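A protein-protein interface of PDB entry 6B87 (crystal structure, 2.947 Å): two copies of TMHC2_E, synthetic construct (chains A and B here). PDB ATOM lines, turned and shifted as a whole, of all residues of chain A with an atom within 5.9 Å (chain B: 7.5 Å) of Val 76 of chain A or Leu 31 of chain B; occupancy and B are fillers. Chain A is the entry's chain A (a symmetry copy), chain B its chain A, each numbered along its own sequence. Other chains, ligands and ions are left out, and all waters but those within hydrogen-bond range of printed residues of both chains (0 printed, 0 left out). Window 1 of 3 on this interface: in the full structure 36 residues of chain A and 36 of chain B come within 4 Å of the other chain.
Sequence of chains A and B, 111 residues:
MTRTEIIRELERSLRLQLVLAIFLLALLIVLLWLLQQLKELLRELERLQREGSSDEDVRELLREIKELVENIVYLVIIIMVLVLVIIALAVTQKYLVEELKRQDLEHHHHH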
ATOM      1  N   LEU A  31      -5.110 -21.484  25.363  1.00  0.00           N
ATOM      2  CA  LEU A  31      -5.997 -20.480  25.923  1.00  0.00           C
ATOM      3  C   LEU A  31      -7.380 -21.041  26.235  1.00  0.00           C
ATOM      4  O   LEU A  31      -7.923 -20.755  27.299  1.00  0.00           O
ATOM      5  CB  LEU A  31      -6.098 -19.303  24.961  1.00  0.00           C
ATOM      6  CG  LEU A  31      -6.994 -18.162  25.401  1.00  0.00           C
ATOM      7  CD1 LEU A  31      -6.503 -17.623  26.723  1.00  0.00           C
ATOM      8  CD2 LEU A  31      -6.954 -17.084  24.332  1.00  0.00           C
ATOM      9  N   LEU A  35      -9.235 -21.446  29.886  1.00  0.00           N
ATOM     10  CA  LEU A  35     -10.599 -20.975  30.108  1.00  0.00           C
ATOM     11  C   LEU A  35     -11.515 -22.089  30.613  1.00  0.00           C
ATOM     12  O   LEU A  35     -12.407 -21.848  31.434  1.00  0.00           O
ATOM     13  CB  LEU A  35     -11.142 -20.382  28.818  1.00  0.00           C
ATOM     14  CG  LEU A  35     -10.477 -19.075  28.388  1.00  0.00           C
ATOM     15  CD1 LEU A  35     -10.940 -18.717  26.989  1.00  0.00           C
ATOM     16  CD2 LEU A  35     -10.835 -17.988  29.393  1.00  0.00           C
ATOM     17  N   ASN A  71      -2.612 -15.565  34.263  1.00  0.00           N
ATOM     18  CA  ASN A  71      -1.904 -16.415  33.305  1.00  0.00           C
ATOM     19  C   ASN A  71      -2.569 -16.340  31.926  1.00  0.00           C
ATOM     20  O   ASN A  71      -1.887 -16.208  30.906  1.00  0.00           O
ATOM     21  CB  ASN A  71      -1.866 -17.858  33.790  1.00  0.00           C
ATOM     22  CG  ASN A  71      -1.013 -18.059  35.025  1.00  0.00           C
ATOM     23  OD1 ASN A  71      -0.305 -17.147  35.467  1.00  0.00           O
ATOM     24  ND2 ASN A  71      -1.055 -19.247  35.582  1.00  0.00           N
ATOM     25  N   ILE A  72      -3.907 -16.360  31.922  1.00  0.00           N
ATOM     26  CA  ILE A  72      -4.722 -16.196  30.726  1.00  0.00           C
ATOM     27  C   ILE A  72      -4.480 -14.877  30.032  1.00  0.00           C
ATOM     28  O   ILE A  72      -4.319 -14.846  28.813  1.00  0.00           O
ATOM     29  CB  ILE A  72      -6.208 -16.327  31.074  1.00  0.00           C
ATOM     30  CG1 ILE A  72      -6.532 -17.777  31.406  1.00  0.00           C
ATOM     31  CG2 ILE A  72      -7.079 -15.803  29.966  1.00  0.00           C
ATOM     32  CD1 ILE A  72      -7.891 -17.987  32.032  1.00  0.00           C
ATOM     33  N   VAL A  73      -4.426 -13.795  30.795  1.00  0.00           N
ATOM     34  CA  VAL A  73      -4.113 -12.496  30.230  1.00  0.00           C
ATOM     35  C   VAL A  73      -2.718 -12.417  29.641  1.00  0.00           C
ATOM     36  O   VAL A  73      -2.553 -11.832  28.570  1.00  0.00           O
ATOM     37  CB  VAL A  73      -4.269 -11.389  31.260  1.00  0.00           C
ATOM     38  CG1 VAL A  73      -3.676 -10.102  30.703  1.00  0.00           C
ATOM     39  CG2 VAL A  73      -5.751 -11.199  31.566  1.00  0.00           C
ATOM     40  N   TYR A  74      -1.714 -12.985  30.327  1.00  0.00           N
ATOM     41  CA  TYR A  74      -0.356 -12.953  29.785  1.00  0.00           C
ATOM     42  C   TYR A  74      -0.261 -13.723  28.481  1.00  0.00           C
ATOM     43  O   TYR A  74       0.348 -13.239  27.531  1.00  0.00           O
ATOM     44  CB  TYR A  74       0.644 -13.511  30.786  1.00  0.00           C
ATOM     45  CG  TYR A  74       0.910 -12.565  31.926  1.00  0.00           C
ATOM     46  CD1 TYR A  74       1.262 -13.050  33.180  1.00  0.00           C
ATOM     47  CD2 TYR A  74       0.784 -11.202  31.716  1.00  0.00           C
ATOM     48  CE1 TYR A  74       1.481 -12.170  34.221  1.00  0.00           C
ATOM     49  CE2 TYR A  74       0.999 -10.324  32.758  1.00  0.00           C
ATOM     50  CZ  TYR A  74       1.341 -10.804  34.007  1.00  0.00           C
ATOM     51  OH  TYR A  74       1.543  -9.926  35.045  1.00  0.00           O
ATOM     52  N   LEU A  75      -0.916 -14.880  28.420  1.00  0.00           N
ATOM     53  CA  LEU A  75      -0.990 -15.659  27.197  1.00  0.00           C
ATOM     54  C   LEU A  75      -1.639 -14.865  26.076  1.00  0.00           C
ATOM     55  O   LEU A  75      -1.115 -14.831  24.965  1.00  0.00           O
ATOM     56  CB  LEU A  75      -1.767 -16.944  27.445  1.00  0.00           C
ATOM     57  CG  LEU A  75      -1.993 -17.839  26.226  1.00  0.00           C
ATOM     58  CD1 LEU A  75      -0.659 -18.285  25.638  1.00  0.00           C
ATOM     59  CD2 LEU A  75      -2.800 -19.043  26.661  1.00  0.00           C
ATOM     60  N   VAL A  76      -2.759 -14.199  26.367  1.00  0.00           N
ATOM     61  CA  VAL A  76      -3.405 -13.346  25.385  1.00  0.00           C
ATOM     62  C   VAL A  76      -2.516 -12.233  24.875  1.00  0.00           C
ATOM     63  O   VAL A  76      -2.490 -11.979  23.672  1.00  0.00           O
ATOM     64  CB  VAL A  76      -4.684 -12.741  25.955  1.00  0.00           C
ATOM     65  CG1 VAL A  76      -5.187 -11.632  25.037  1.00  0.00           C
ATOM     66  CG2 VAL A  76      -5.730 -13.845  26.055  1.00  0.00           C
ATOM     67  N   ILE A  77      -1.785 -11.567  25.759  1.00  0.00           N
ATOM     68  CA  ILE A  77      -0.879 -10.517  25.315  1.00  0.00           C
ATOM     69  C   ILE A  77       0.210 -11.080  24.407  1.00  0.00           C
ATOM     70  O   ILE A  77       0.543 -10.461  23.396  1.00  0.00           O
ATOM     71  CB  ILE A  77      -0.259  -9.776  26.496  1.00  0.00           C
ATOM     72  CG1 ILE A  77      -1.349  -8.982  27.223  1.00  0.00           C
ATOM     73  CG2 ILE A  77       0.833  -8.845  25.990  1.00  0.00           C
ATOM     74  CD1 ILE A  77      -0.935  -8.446  28.569  1.00  0.00           C
ATOM     75  N   ILE A  78       0.741 -12.255  24.751  1.00  0.00           N
ATOM     76  CA  ILE A  78       1.736 -12.942  23.917  1.00  0.00           C
ATOM     77  C   ILE A  78       1.176 -13.219  22.523  1.00  0.00           C
ATOM     78  O   ILE A  78       1.840 -12.950  21.516  1.00  0.00           O
ATOM     79  CB  ILE A  78       2.178 -14.268  24.588  1.00  0.00           C
ATOM     80  CG1 ILE A  78       3.004 -13.962  25.850  1.00  0.00           C
ATOM     81  CG2 ILE A  78       2.957 -15.130  23.602  1.00  0.00           C
ATOM     82  CD1 ILE A  78       3.162 -15.126  26.799  1.00  0.00           C
ATOM     83  N   ILE A  79      -0.062 -13.709  22.475  1.00  0.00           N
ATOM     84  CA  ILE A  79      -0.777 -13.943  21.225  1.00  0.00           C
ATOM     85  C   ILE A  79      -0.929 -12.658  20.401  1.00  0.00           C
ATOM     86  O   ILE A  79      -0.702 -12.681  19.195  1.00  0.00           O
ATOM     87  CB  ILE A  79      -2.151 -14.596  21.522  1.00  0.00           C
ATOM     88  CG1 ILE A  79      -1.949 -16.037  21.990  1.00  0.00           C
ATOM     89  CG2 ILE A  79      -3.074 -14.536  20.343  1.00  0.00           C
ATOM     90  CD1 ILE A  79      -3.189 -16.685  22.565  1.00  0.00           C
ATOM     91  N   MET A  80      -1.261 -11.539  21.049  1.00  0.00           N
ATOM     92  CA  MET A  80      -1.362 -10.258  20.356  1.00  0.00           C
ATOM     93  C   MET A  80      -0.056  -9.817  19.746  1.00  0.00           C
ATOM     94  O   MET A  80      -0.049  -9.272  18.644  1.00  0.00           O
ATOM     95  CB  MET A  80      -1.842  -9.163  21.299  1.00  0.00           C
ATOM     96  CG  MET A  80      -3.289  -9.286  21.721  1.00  0.00           C
ATOM     97  SD  MET A  80      -3.768  -8.027  22.909  1.00  0.00           S
ATOM     98  CE  MET A  80      -3.729  -6.588  21.839  1.00  0.00           C
ATOM     99  N   VAL A  81       1.051 -10.053  20.459  1.00  0.00           N
ATOM    100  CA  VAL A  81       2.373  -9.694  19.954  1.00  0.00           C
ATOM    101  C   VAL A  81       2.748 -10.560  18.754  1.00  0.00           C
ATOM    102  O   VAL A  81       3.233 -10.048  17.744  1.00  0.00           O
ATOM    103  CB  VAL A  81       3.433  -9.827  21.045  1.00  0.00           C
ATOM    104  CG1 VAL A  81       4.802  -9.610  20.433  1.00  0.00           C
ATOM    105  CG2 VAL A  81       3.185  -8.810  22.150  1.00  0.00           C
ATOM    106  N   LEU B  24      -8.456  -9.838  13.743  1.00  0.00           N
ATOM    107  CA  LEU B  24      -8.021 -10.633  14.900  1.00  0.00           C
ATOM    108  C   LEU B  24      -7.517  -9.770  15.998  1.00  0.00           C
ATOM    109  O   LEU B  24      -7.851  -9.998  17.156  1.00  0.00           O
ATOM    110  CB  LEU B  24      -6.850 -11.589  14.613  1.00  0.00           C
ATOM    111  CG  LEU B  24      -7.092 -12.851  13.808  1.00  0.00           C
ATOM    112  CD1 LEU B  24      -5.747 -13.518  13.566  1.00  0.00           C
ATOM    113  CD2 LEU B  24      -7.985 -13.778  14.595  1.00  0.00           C
ATOM    114  N   LEU B  25      -6.700  -8.786  15.649  1.00  0.00           N
ATOM    115  CA  LEU B  25      -6.095  -7.958  16.664  1.00  0.00           C
ATOM    116  C   LEU B  25      -7.160  -7.187  17.431  1.00  0.00           C
ATOM    117  O   LEU B  25      -7.088  -7.071  18.654  1.00  0.00           O
ATOM    118  CB  LEU B  25      -5.096  -7.015  16.036  1.00  0.00           C
ATOM    119  CG  LEU B  25      -4.251  -6.254  17.048  1.00  0.00           C
ATOM    120  CD1 LEU B  25      -3.484  -7.268  17.901  1.00  0.00           C
ATOM    121  CD2 LEU B  25      -3.304  -5.329  16.307  1.00  0.00           C
ATOM    122  N   ALA B  26      -8.174  -6.704  16.711  1.00  0.00           N
ATOM    123  CA  ALA B  26      -9.318  -6.044  17.322  1.00  0.00           C
ATOM    124  C   ALA B  26     -10.099  -6.995  18.225  1.00  0.00           C
ATOM    125  O   ALA B  26     -10.459  -6.624  19.340  1.00  0.00           O
ATOM    126  CB  ALA B  26     -10.216  -5.498  16.241  1.00  0.00           C
ATOM    127  N   LEU B  27     -10.323  -8.230  17.764  1.00  0.00           N
ATOM    128  CA  LEU B  27     -11.005  -9.245  18.562  1.00  0.00           C
ATOM    129  C   LEU B  27     -10.220  -9.589  19.828  1.00  0.00           C
ATOM    130  O   LEU B  27     -10.820  -9.802  20.881  1.00  0.00           O
ATOM    131  CB  LEU B  27     -11.220 -10.521  17.733  1.00  0.00           C
ATOM    132  CG  LEU B  27     -12.249 -10.442  16.585  1.00  0.00           C
ATOM    133  CD1 LEU B  27     -12.166 -11.718  15.737  1.00  0.00           C
ATOM    134  CD2 LEU B  27     -13.653 -10.261  17.157  1.00  0.00           C
ATOM    135  N   LEU B  28      -8.883  -9.614  19.725  1.00  0.00           N
ATOM    136  CA  LEU B  28      -8.009  -9.855  20.866  1.00  0.00           C
ATOM    137  C   LEU B  28      -8.057  -8.706  21.874  1.00  0.00           C
ATOM    138  O   LEU B  28      -8.029  -8.943  23.081  1.00  0.00           O
ATOM    139  CB  LEU B  28      -6.568 -10.063  20.386  1.00  0.00           C
ATOM    140  CG  LEU B  28      -6.300 -11.363  19.601  1.00  0.00           C
ATOM    141  CD1 LEU B  28      -4.903 -11.319  18.990  1.00  0.00           C
ATOM    142  CD2 LEU B  28      -6.439 -12.550  20.539  1.00  0.00           C
ATOM    143  N   ILE B  29      -8.176  -7.472  21.386  1.00  0.00           N
ATOM    144  CA  ILE B  29      -8.389  -6.322  22.264  1.00  0.00           C
ATOM    145  C   ILE B  29      -9.748  -6.394  22.989  1.00  0.00           C
ATOM    146  O   ILE B  29      -9.841  -6.055  24.170  1.00  0.00           O
ATOM    147  CB  ILE B  29      -8.253  -5.007  21.491  1.00  0.00           C
ATOM    148  CG1 ILE B  29      -6.791  -4.818  21.079  1.00  0.00           C
ATOM    149  CG2 ILE B  29      -8.736  -3.853  22.345  1.00  0.00           C
ATOM    150  CD1 ILE B  29      -6.573  -3.709  20.084  1.00  0.00           C
ATOM    151  N   VAL B  30     -10.792  -6.852  22.293  1.00  0.00           N
ATOM    152  CA  VAL B  30     -12.073  -7.113  22.947  1.00  0.00           C
ATOM    153  C   VAL B  30     -11.931  -8.209  23.995  1.00  0.00           C
ATOM    154  O   VAL B  30     -12.470  -8.092  25.094  1.00  0.00           O
ATOM    155  CB  VAL B  30     -13.154  -7.527  21.935  1.00  0.00           C
ATOM    156  CG1 VAL B  30     -14.398  -8.003  22.679  1.00  0.00           C
ATOM    157  CG2 VAL B  30     -13.487  -6.344  21.045  1.00  0.00           C
ATOM    158  N   LEU B  31     -11.201  -9.260  23.649  1.00  0.00           N
ATOM    159  CA  LEU B  31     -10.925 -10.363  24.551  1.00  0.00           C
ATOM    160  C   LEU B  31     -10.199  -9.908  25.812  1.00  0.00           C
ATOM    161  O   LEU B  31     -10.556 -10.340  26.906  1.00  0.00           O
ATOM    162  CB  LEU B  31     -10.116 -11.425  23.817  1.00  0.00           C
ATOM    163  CG  LEU B  31      -9.742 -12.651  24.627  1.00  0.00           C
ATOM    164  CD1 LEU B  31     -10.998 -13.314  25.138  1.00  0.00           C
ATOM    165  CD2 LEU B  31      -8.961 -13.596  23.731  1.00  0.00           C
ATOM    166  N   LEU B  32      -9.209  -9.017  25.673  1.00  0.00           N
ATOM    167  CA  LEU B  32      -8.602  -8.414  26.852  1.00  0.00           C
ATOM    168  C   LEU B  32      -9.566  -7.608  27.668  1.00  0.00           C
ATOM    169  O   LEU B  32      -9.529  -7.700  28.892  1.00  0.00           O
ATOM    170  CB  LEU B  32      -7.427  -7.508  26.511  1.00  0.00           C
ATOM    171  CG  LEU B  32      -6.121  -8.212  26.212  1.00  0.00           C
ATOM    172  CD1 LEU B  32      -5.078  -7.179  25.797  1.00  0.00           C
ATOM    173  CD2 LEU B  32      -5.693  -8.959  27.477  1.00  0.00           C
ATOM    174  N   TRP B  33     -10.437  -6.838  27.013  1.00  0.00           N
ATOM    175  CA  TRP B  33     -11.434  -6.063  27.730  1.00  0.00           C
ATOM    176  C   TRP B  33     -12.299  -7.004  28.583  1.00  0.00           C
ATOM    177  O   TRP B  33     -12.508  -6.745  29.766  1.00  0.00           O
ATOM    178  CB  TRP B  33     -12.275  -5.249  26.735  1.00  0.00           C
ATOM    179  CG  TRP B  33     -13.268  -4.302  27.355  1.00  0.00           C
ATOM    180  CD1 TRP B  33     -13.011  -3.040  27.801  1.00  0.00           C
ATOM    181  CD2 TRP B  33     -14.682  -4.526  27.582  1.00  0.00           C
ATOM    182  NE1 TRP B  33     -14.156  -2.468  28.296  1.00  0.00           N
ATOM    183  CE2 TRP B  33     -15.189  -3.364  28.172  1.00  0.00           C
ATOM    184  CE3 TRP B  33     -15.542  -5.602  27.339  1.00  0.00           C
ATOM    185  CZ2 TRP B  33     -16.524  -3.246  28.529  1.00  0.00           C
ATOM    186  CZ3 TRP B  33     -16.880  -5.483  27.696  1.00  0.00           C
ATOM    187  CH2 TRP B  33     -17.358  -4.335  28.277  1.00  0.00           C
ATOM    188  N   LEU B  34     -12.737  -8.124  28.001  1.00  0.00           N
ATOM    189  CA  LEU B  34     -13.543  -9.107  28.724  1.00  0.00           C
ATOM    190  C   LEU B  34     -12.790  -9.760  29.893  1.00  0.00           C
ATOM    191  O   LEU B  34     -13.373 -10.022  30.944  1.00  0.00           O
ATOM    192  CB  LEU B  34     -13.995 -10.213  27.775  1.00  0.00           C
ATOM    193  CG  LEU B  34     -14.971  -9.827  26.656  1.00  0.00           C
ATOM    194  CD1 LEU B  34     -15.198 -11.049  25.773  1.00  0.00           C
ATOM    195  CD2 LEU B  34     -16.274  -9.332  27.256  1.00  0.00           C
ATOM    196  N   LEU B  35     -11.497 -10.015  29.716  1.00  0.00           N
ATOM    197  CA  LEU B  35     -10.672 -10.574  30.783  1.00  0.00           C
ATOM    198  C   LEU B  35     -10.437  -9.570  31.912  1.00  0.00           C
ATOM    199  O   LEU B  35     -10.379  -9.947  33.086  1.00  0.00           O
ATOM    200  CB  LEU B  35      -9.347 -11.039  30.200  1.00  0.00           C
ATOM    201  CG  LEU B  35      -9.448 -12.255  29.279  1.00  0.00           C
ATOM    202  CD1 LEU B  35      -8.114 -12.472  28.592  1.00  0.00           C
ATOM    203  CD2 LEU B  35      -9.855 -13.466  30.108  1.00  0.00           C
ATOM    204  N   GLN B  36     -10.346  -8.291  31.555  1.00  0.00           N
ATOM    205  CA  GLN B  36     -10.256  -7.218  32.534  1.00  0.00           C
ATOM    206  C   GLN B  36     -11.581  -7.091  33.307  1.00  0.00           C
ATOM    207  O   GLN B  36     -11.573  -6.794  34.504  1.00  0.00           O
ATOM    208  CB  GLN B  36      -9.864  -5.910  31.836  1.00  0.00           C
ATOM    209  CG  GLN B  36      -8.420  -5.922  31.318  1.00  0.00           C
ATOM    210  CD  GLN B  36      -8.080  -4.759  30.386  1.00  0.00           C
ATOM    211  OE1 GLN B  36      -8.948  -3.987  29.972  1.00  0.00           O
ATOM    212  NE2 GLN B  36      -6.800  -4.636  30.042  1.00  0.00           N
ATOM    213  N   GLN B  37     -12.711  -7.380  32.637  1.00  0.00           N
ATOM    214  CA  GLN B  37     -14.009  -7.436  33.311  1.00  0.00           C
ATOM    215  C   GLN B  37     -14.050  -8.585  34.353  1.00  0.00           C
ATOM    216  O   GLN B  37     -14.617  -8.405  35.430  1.00  0.00           O
ATOM    217  CB  GLN B  37     -15.157  -7.591  32.286  1.00  0.00           C
ATOM    218  CG  GLN B  37     -15.358  -6.402  31.344  1.00  0.00           C
ATOM    219  CD  GLN B  37     -15.842  -5.147  32.040  1.00  0.00           C
ATOM    220  OE1 GLN B  37     -16.915  -5.141  32.650  1.00  0.00           O
ATOM    221  NE2 GLN B  37     -15.054  -4.078  31.962  1.00  0.00           N
ATOM    222  N   ASN B  71     -18.980 -16.036  27.398  1.00  0.00           N
ATOM    223  CA  ASN B  71     -18.840 -15.048  26.327  1.00  0.00           C
ATOM    224  C   ASN B  71     -17.392 -14.996  25.829  1.00  0.00           C
ATOM    225  O   ASN B  71     -17.143 -14.977  24.620  1.00  0.00           O
ATOM    226  CB  ASN B  71     -19.280 -13.670  26.803  1.00  0.00           C
ATOM    227  CG  ASN B  71     -20.766 -13.572  27.082  1.00  0.00           C
ATOM    228  OD1 ASN B  71     -21.534 -14.494  26.784  1.00  0.00           O
ATOM    229  ND2 ASN B  71     -21.187 -12.459  27.637  1.00  0.00           N
ATOM    230  N   ILE B  72     -16.448 -15.040  26.775  1.00  0.00           N
ATOM    231  CA  ILE B  72     -15.019 -15.104  26.501  1.00  0.00           C
ATOM    232  C   ILE B  72     -14.635 -16.322  25.694  1.00  0.00           C
ATOM    233  O   ILE B  72     -13.883 -16.205  24.728  1.00  0.00           O
ATOM    234  CB  ILE B  72     -14.225 -15.086  27.811  1.00  0.00           C
ATOM    235  CG1 ILE B  72     -14.302 -13.700  28.439  1.00  0.00           C
ATOM    236  CG2 ILE B  72     -12.802 -15.521  27.596  1.00  0.00           C
ATOM    237  CD1 ILE B  72     -13.798 -13.629  29.861  1.00  0.00           C
ATOM    238  N   VAL B  73     -15.161 -17.480  26.064  1.00  0.00           N
ATOM    239  CA  VAL B  73     -14.919 -18.689  25.299  1.00  0.00           C
ATOM    240  C   VAL B  73     -15.480 -18.633  23.892  1.00  0.00           C
ATOM    241  O   VAL B  73     -14.810 -19.082  22.962  1.00  0.00           O
ATOM    242  CB  VAL B  73     -15.486 -19.914  26.000  1.00  0.00           C
ATOM    243  CG1 VAL B  73     -15.447 -21.098  25.044  1.00  0.00           C
ATOM    244  CG2 VAL B  73     -14.650 -20.208  27.241  1.00  0.00           C
ATOM    245  N   LEU B  75     -16.003 -15.962  22.048  1.00  0.00           N
ATOM    246  CA  LEU B  75     -15.122 -15.052  21.338  1.00  0.00           C
ATOM    247  C   LEU B  75     -13.833 -15.742  20.926  1.00  0.00           C
ATOM    248  O   LEU B  75     -13.414 -15.623  19.777  1.00  0.00           O
ATOM    249  CB  LEU B  75     -14.812 -13.843  22.209  1.00  0.00           C
ATOM    250  CG  LEU B  75     -13.833 -12.826  21.623  1.00  0.00           C
ATOM    251  CD1 LEU B  75     -14.377 -12.251  20.320  1.00  0.00           C
ATOM    252  CD2 LEU B  75     -13.630 -11.721  22.636  1.00  0.00           C
ATOM    253  N   VAL B  76     -13.219 -16.491  21.845  1.00  0.00           N
ATOM    254  CA  VAL B  76     -12.027 -17.255  21.521  1.00  0.00           C
ATOM    255  C   VAL B  76     -12.239 -18.258  20.407  1.00  0.00           C
ATOM    256  O   VAL B  76     -11.393 -18.370  19.522  1.00  0.00           O
ATOM    257  CB  VAL B  76     -11.501 -17.982  22.753  1.00  0.00           C
ATOM    258  CG1 VAL B  76     -10.443 -19.001  22.343  1.00  0.00           C
ATOM    259  CG2 VAL B  76     -10.888 -16.949  23.692  1.00  0.00           C
ATOM    260  N   ILE B  79     -12.338 -16.400  17.168  1.00  0.00           N
ATOM    261  CA  ILE B  79     -10.960 -16.059  16.831  1.00  0.00           C
ATOM    262  C   ILE B  79     -10.208 -17.246  16.216  1.00  0.00           C
ATOM    263  O   ILE B  79      -9.515 -17.074  15.219  1.00  0.00           O
ATOM    264  CB  ILE B  79     -10.234 -15.510  18.086  1.00  0.00           C
ATOM    265  CG1 ILE B  79     -10.778 -14.125  18.434  1.00  0.00           C
ATOM    266  CG2 ILE B  79      -8.746 -15.479  17.911  1.00  0.00           C
ATOM    267  CD1 ILE B  79     -10.342 -13.607  19.788  1.00  0.00           C
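Val 76 of chain B touches Leu 31 of chain A.
CD2 of Leu 35 of chain A touches CG2 of Ile 72 of chain B, 3.6 Å away.
Val 73 of chain B touches Leu 35 of chain A (CG2 to CB, 3.9 Å).
Val 76 of chain B touches Leu 35 of chain A.
CG2 of Val 73 of chain A touches CB of Leu 35 of chain B (3.9 Å).
Leu 31 of chain B touches Val 76 of chain A (CD2 to CG2, 3.99 Å).
CD2 of Leu 32 of chain B touches CG1 of Val 76 of chain A, at 3.7 Å.
Leu 35 of chain B touches Val 76 of chain A (CD1 to CG2, 3.7 Å).
Leu 28 of chain B touches Ile 79 of chain A (CD2 to CG2, 3.9 Å).
Met 80 of chain A touches Leu 28 of chain B.
Printed residues of chain A within 4 Å of Leu 28 of chain B: Ile 79 and Met 80.
Of the printed residues of chain A, Ile 29 of chain B touches Met 80 (3.6 Å).
Printed residues of chain A within 4 Å of Leu 31 of chain B: Val 76 (3.99 Å).
Of the printed residues of chain A, Ile 72 of chain B touches Leu 35.
Printed residues of chain A within 4 Å of Val 76 of chain B: Leu 31 (3.99 Å) and Leu 35 (3.7 Å).
The nearest printed residue of chain B that does not touch Val 76 of chain A is Leu 28 of chain B (4.4 Å).
Of the 20 printed residues of chain B, 8 touch a printed residue of chain A.
Of the 13 printed residues of chain A, 7 touch a printed residue of chain B.
Printed residues of chain A that touch a printed residue of chain B: Leu 31, Leu 35, Ile 72, Val 73, Val 76, Ile 79 and Met 80.
Hydrophobic or aromatic side chains of chain A within 4 Å of the printed part of chain B: Leu 31, Leu 35, Ile 72, Val 73, Val 76, Ile 79 and Met 80.
Among the printed residues, 14 pairs touch across the chains.
Among the printed residues, no Asp or Glu carboxylate lies within 4 Å of a Lys or Arg side-chain nitrogen of the other chain.
Leu 31 of chain A touches Val 76 of chain B, and with the chains exchanged Val 76 of chain A touches Leu 31 of chain B.
Leu 35 of chain A touches Ile 72 of chain B, and with the chains exchanged Ile 72 of chain A touches Leu 35 of chain B.
Leu 35 of chain A touches Val 73 of chain B, and with the chains exchanged Val 73 of chain A touches Leu 35 of chain B.
Leu 35 of chain A touches Val 76 of chain B, and with the chains exchanged Val 76 of chain A touches Leu 35 of chain B.
Of the 14 pairs that touch across the chains among the printed residues, 8 have their exchanged pair printed and touching as well.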
